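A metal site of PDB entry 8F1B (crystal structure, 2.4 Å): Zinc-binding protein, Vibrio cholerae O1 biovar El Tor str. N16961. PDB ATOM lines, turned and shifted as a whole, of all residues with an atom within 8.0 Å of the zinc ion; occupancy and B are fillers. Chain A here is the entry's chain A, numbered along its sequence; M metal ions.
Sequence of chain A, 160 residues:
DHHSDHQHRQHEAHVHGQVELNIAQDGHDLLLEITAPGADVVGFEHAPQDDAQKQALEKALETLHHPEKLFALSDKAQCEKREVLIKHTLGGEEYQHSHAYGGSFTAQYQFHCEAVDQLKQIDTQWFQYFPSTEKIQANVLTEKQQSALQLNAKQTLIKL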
ATOM      1  N   LYS A  59     -14.875 -20.182  37.266  1.00  0.00           N
ATOM      2  CA  LYS A  59     -14.333 -21.174  36.302  1.00  0.00           C
ATOM      3  C   LYS A  59     -14.642 -20.690  34.876  1.00  0.00           C
ATOM      4  O   LYS A  59     -13.698 -20.639  34.051  1.00  0.00           O
ATOM      5  CB  LYS A  59     -14.895 -22.571  36.560  1.00  0.00           C
ATOM      6  CG  LYS A  59     -13.963 -23.697  36.100  1.00  0.00           C
ATOM      7  CD  LYS A  59     -14.593 -25.071  35.988  1.00  0.00           C
ATOM      8  CE  LYS A  59     -14.870 -25.486  34.563  1.00  0.00           C
ATOM      9  NZ  LYS A  59     -15.701 -26.723  34.487  1.00  0.00           N
ATOM     10  N   LEU A  61     -15.440 -17.561  33.690  1.00  0.00           N
ATOM     11  CA  LEU A  61     -14.761 -16.298  33.318  1.00  0.00           C
ATOM     12  C   LEU A  61     -13.286 -16.592  33.039  1.00  0.00           C
ATOM     13  O   LEU A  61     -12.734 -16.011  32.112  1.00  0.00           O
ATOM     14  CB  LEU A  61     -14.921 -15.260  34.434  1.00  0.00           C
ATOM     15  CG  LEU A  61     -16.297 -14.603  34.461  1.00  0.00           C
ATOM     16  CD1 LEU A  61     -16.578 -13.954  35.814  1.00  0.00           C
ATOM     17  CD2 LEU A  61     -16.441 -13.596  33.317  1.00  0.00           C
ATOM     18  N   GLU A  62     -12.702 -17.477  33.815  1.00  0.00           N
ATOM     19  CA  GLU A  62     -11.285 -17.854  33.634  1.00  0.00           C
ATOM     20  C   GLU A  62     -11.154 -18.624  32.308  1.00  0.00           C
ATOM     21  O   GLU A  62     -10.137 -18.449  31.631  1.00  0.00           O
ATOM     22  CB  GLU A  62     -10.798 -18.628  34.857  1.00  0.00           C
ATOM     23  CG  GLU A  62      -9.291 -18.821  34.884  1.00  0.00           C
ATOM     24  CD  GLU A  62      -8.811 -19.973  34.003  1.00  0.00           C
ATOM     25  OE1 GLU A  62      -9.616 -20.886  33.769  1.00  0.00           O
ATOM     26  OE2 GLU A  62      -7.663 -19.939  33.554  1.00  0.00           O
ATOM     27  N   THR A  63     -12.119 -19.458  31.972  1.00  0.00           N
ATOM     28  CA  THR A  63     -12.103 -20.233  30.704  1.00  0.00           C
ATOM     29  C   THR A  63     -12.175 -19.278  29.507  1.00  0.00           C
ATOM     30  O   THR A  63     -11.431 -19.505  28.526  1.00  0.00           O
ATOM     31  CB  THR A  63     -13.266 -21.214  30.602  1.00  0.00           C
ATOM     32  OG1 THR A  63     -13.030 -22.209  31.604  1.00  0.00           O
ATOM     33  CG2 THR A  63     -13.362 -21.844  29.235  1.00  0.00           C
ATOM     34  N   LEU A  64     -13.024 -18.263  29.606  1.00  0.00           N
ATOM     35  CA  LEU A  64     -13.345 -17.385  28.456  1.00  0.00           C
ATOM     36  C   LEU A  64     -12.127 -16.564  28.032  1.00  0.00           C
ATOM     37  O   LEU A  64     -12.197 -15.987  26.956  1.00  0.00           O
ATOM     38  CB  LEU A  64     -14.499 -16.457  28.843  1.00  0.00           C
ATOM     39  CG  LEU A  64     -15.895 -17.055  28.758  1.00  0.00           C
ATOM     40  CD1 LEU A  64     -16.948 -15.988  29.041  1.00  0.00           C
ATOM     41  CD2 LEU A  64     -16.154 -17.668  27.389  1.00  0.00           C
ATOM     42  N   HIS A  65     -11.064 -16.482  28.829  1.00  0.00           N
ATOM     43  CA  HIS A  65      -9.850 -15.721  28.426  1.00  0.00           C
ATOM     44  C   HIS A  65      -8.798 -16.677  27.840  1.00  0.00           C
ATOM     45  O   HIS A  65      -7.662 -16.286  27.695  1.00  0.00           O
ATOM     46  CB  HIS A  65      -9.335 -14.812  29.548  1.00  0.00           C
ATOM     47  CG  HIS A  65      -8.648 -15.515  30.669  1.00  0.00           C
ATOM     48  ND1 HIS A  65      -8.908 -15.206  31.982  1.00  0.00           N
ATOM     49  CD2 HIS A  65      -7.716 -16.504  30.681  1.00  0.00           C
ATOM     50  CE1 HIS A  65      -8.176 -15.970  32.756  1.00  0.00           C
ATOM     51  NE2 HIS A  65      -7.443 -16.773  32.002  1.00  0.00           N
ATOM     52  N   HIS A  66      -9.199 -17.895  27.477  1.00  0.00           N
ATOM     53  CA  HIS A  66      -8.321 -18.851  26.767  1.00  0.00           C
ATOM     54  C   HIS A  66      -8.984 -19.233  25.463  1.00  0.00           C
ATOM     55  O   HIS A  66      -9.395 -20.363  25.299  1.00  0.00           O
ATOM     56  CB  HIS A  66      -8.025 -20.060  27.652  1.00  0.00           C
ATOM     57  CG  HIS A  66      -7.231 -19.733  28.863  1.00  0.00           C
ATOM     58  ND1 HIS A  66      -5.955 -19.251  28.797  1.00  0.00           N
ATOM     59  CD2 HIS A  66      -7.521 -19.839  30.178  1.00  0.00           C
ATOM     60  CE1 HIS A  66      -5.489 -19.053  30.022  1.00  0.00           C
ATOM     61  NE2 HIS A  66      -6.430 -19.407  30.888  1.00  0.00           N
ATOM     62  N   GLU A  68      -7.543 -19.781  22.878  1.00  0.00           N
ATOM     63  CA  GLU A  68      -6.603 -20.771  22.292  1.00  0.00           C
ATOM     64  C   GLU A  68      -6.957 -22.163  22.813  1.00  0.00           C
ATOM     65  O   GLU A  68      -6.516 -23.147  22.185  1.00  0.00           O
ATOM     66  CB  GLU A  68      -5.157 -20.355  22.551  1.00  0.00           C
ATOM     67  CG  GLU A  68      -4.668 -20.686  23.934  1.00  0.00           C
ATOM     68  CD  GLU A  68      -5.124 -19.739  25.040  1.00  0.00           C
ATOM     69  OE1 GLU A  68      -5.919 -18.792  24.739  1.00  0.00           O
ATOM     70  OE2 GLU A  68      -4.668 -19.947  26.191  1.00  0.00           O
ATOM     71  N   LYS A  69      -7.719 -22.281  23.902  1.00  0.00           N
ATOM     72  CA  LYS A  69      -8.309 -23.569  24.326  1.00  0.00           C
ATOM     73  C   LYS A  69      -9.677 -23.765  23.681  1.00  0.00           C
ATOM     74  O   LYS A  69     -10.050 -24.910  23.434  1.00  0.00           O
ATOM     75  CB  LYS A  69      -8.539 -23.648  25.832  1.00  0.00           C
ATOM     76  CG  LYS A  69      -7.300 -23.611  26.697  1.00  0.00           C
ATOM     77  CD  LYS A  69      -7.634 -24.078  28.109  1.00  0.00           C
ATOM     78  CE  LYS A  69      -6.997 -23.283  29.225  1.00  0.00           C
ATOM     79  NZ  LYS A  69      -5.521 -23.383  29.183  1.00  0.00           N
ATOM     80  N   LYS A  81      -2.257 -14.519  20.528  1.00  0.00           N
ATOM     81  CA  LYS A  81      -3.455 -13.798  21.038  1.00  0.00           C
ATOM     82  C   LYS A  81      -3.116 -12.310  21.086  1.00  0.00           C
ATOM     83  O   LYS A  81      -2.062 -11.957  21.658  1.00  0.00           O
ATOM     84  CB  LYS A  81      -3.910 -14.264  22.418  1.00  0.00           C
ATOM     85  CG  LYS A  81      -3.962 -15.758  22.598  1.00  0.00           C
ATOM     86  CD  LYS A  81      -3.698 -16.167  24.027  1.00  0.00           C
ATOM     87  CE  LYS A  81      -4.664 -15.502  24.991  1.00  0.00           C
ATOM     88  NZ  LYS A  81      -4.500 -16.055  26.364  1.00  0.00           N
HETATM   89 ZN    ZN M   1      -6.556 -18.467  32.673  1.00  0.00          ZN
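Three residues have an atom within 4 Å of the zinc ion: Glu 62, His 65 and His 66. Along chain A the residues within 4 Å of the zinc ion span positions 62 to 66. The nearest printed residue that does not touch the zinc ion is Thr 63 (5.7 Å).
NZ of Lys 81 is in hydrogen-bond range of O of His 65, 3.4 Å away. ND1 of His 66 lies within hydrogen-bond range of OE2 of Glu 68 (3.0 Å).
The zinc ion is bound by a ring nitrogen (NE2) of His 66 (2.0 Å), a ring nitrogen (NE2) of His 65 (2.0 Å) and the side-chain carboxylate of Glu 62 (2.0 Å).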
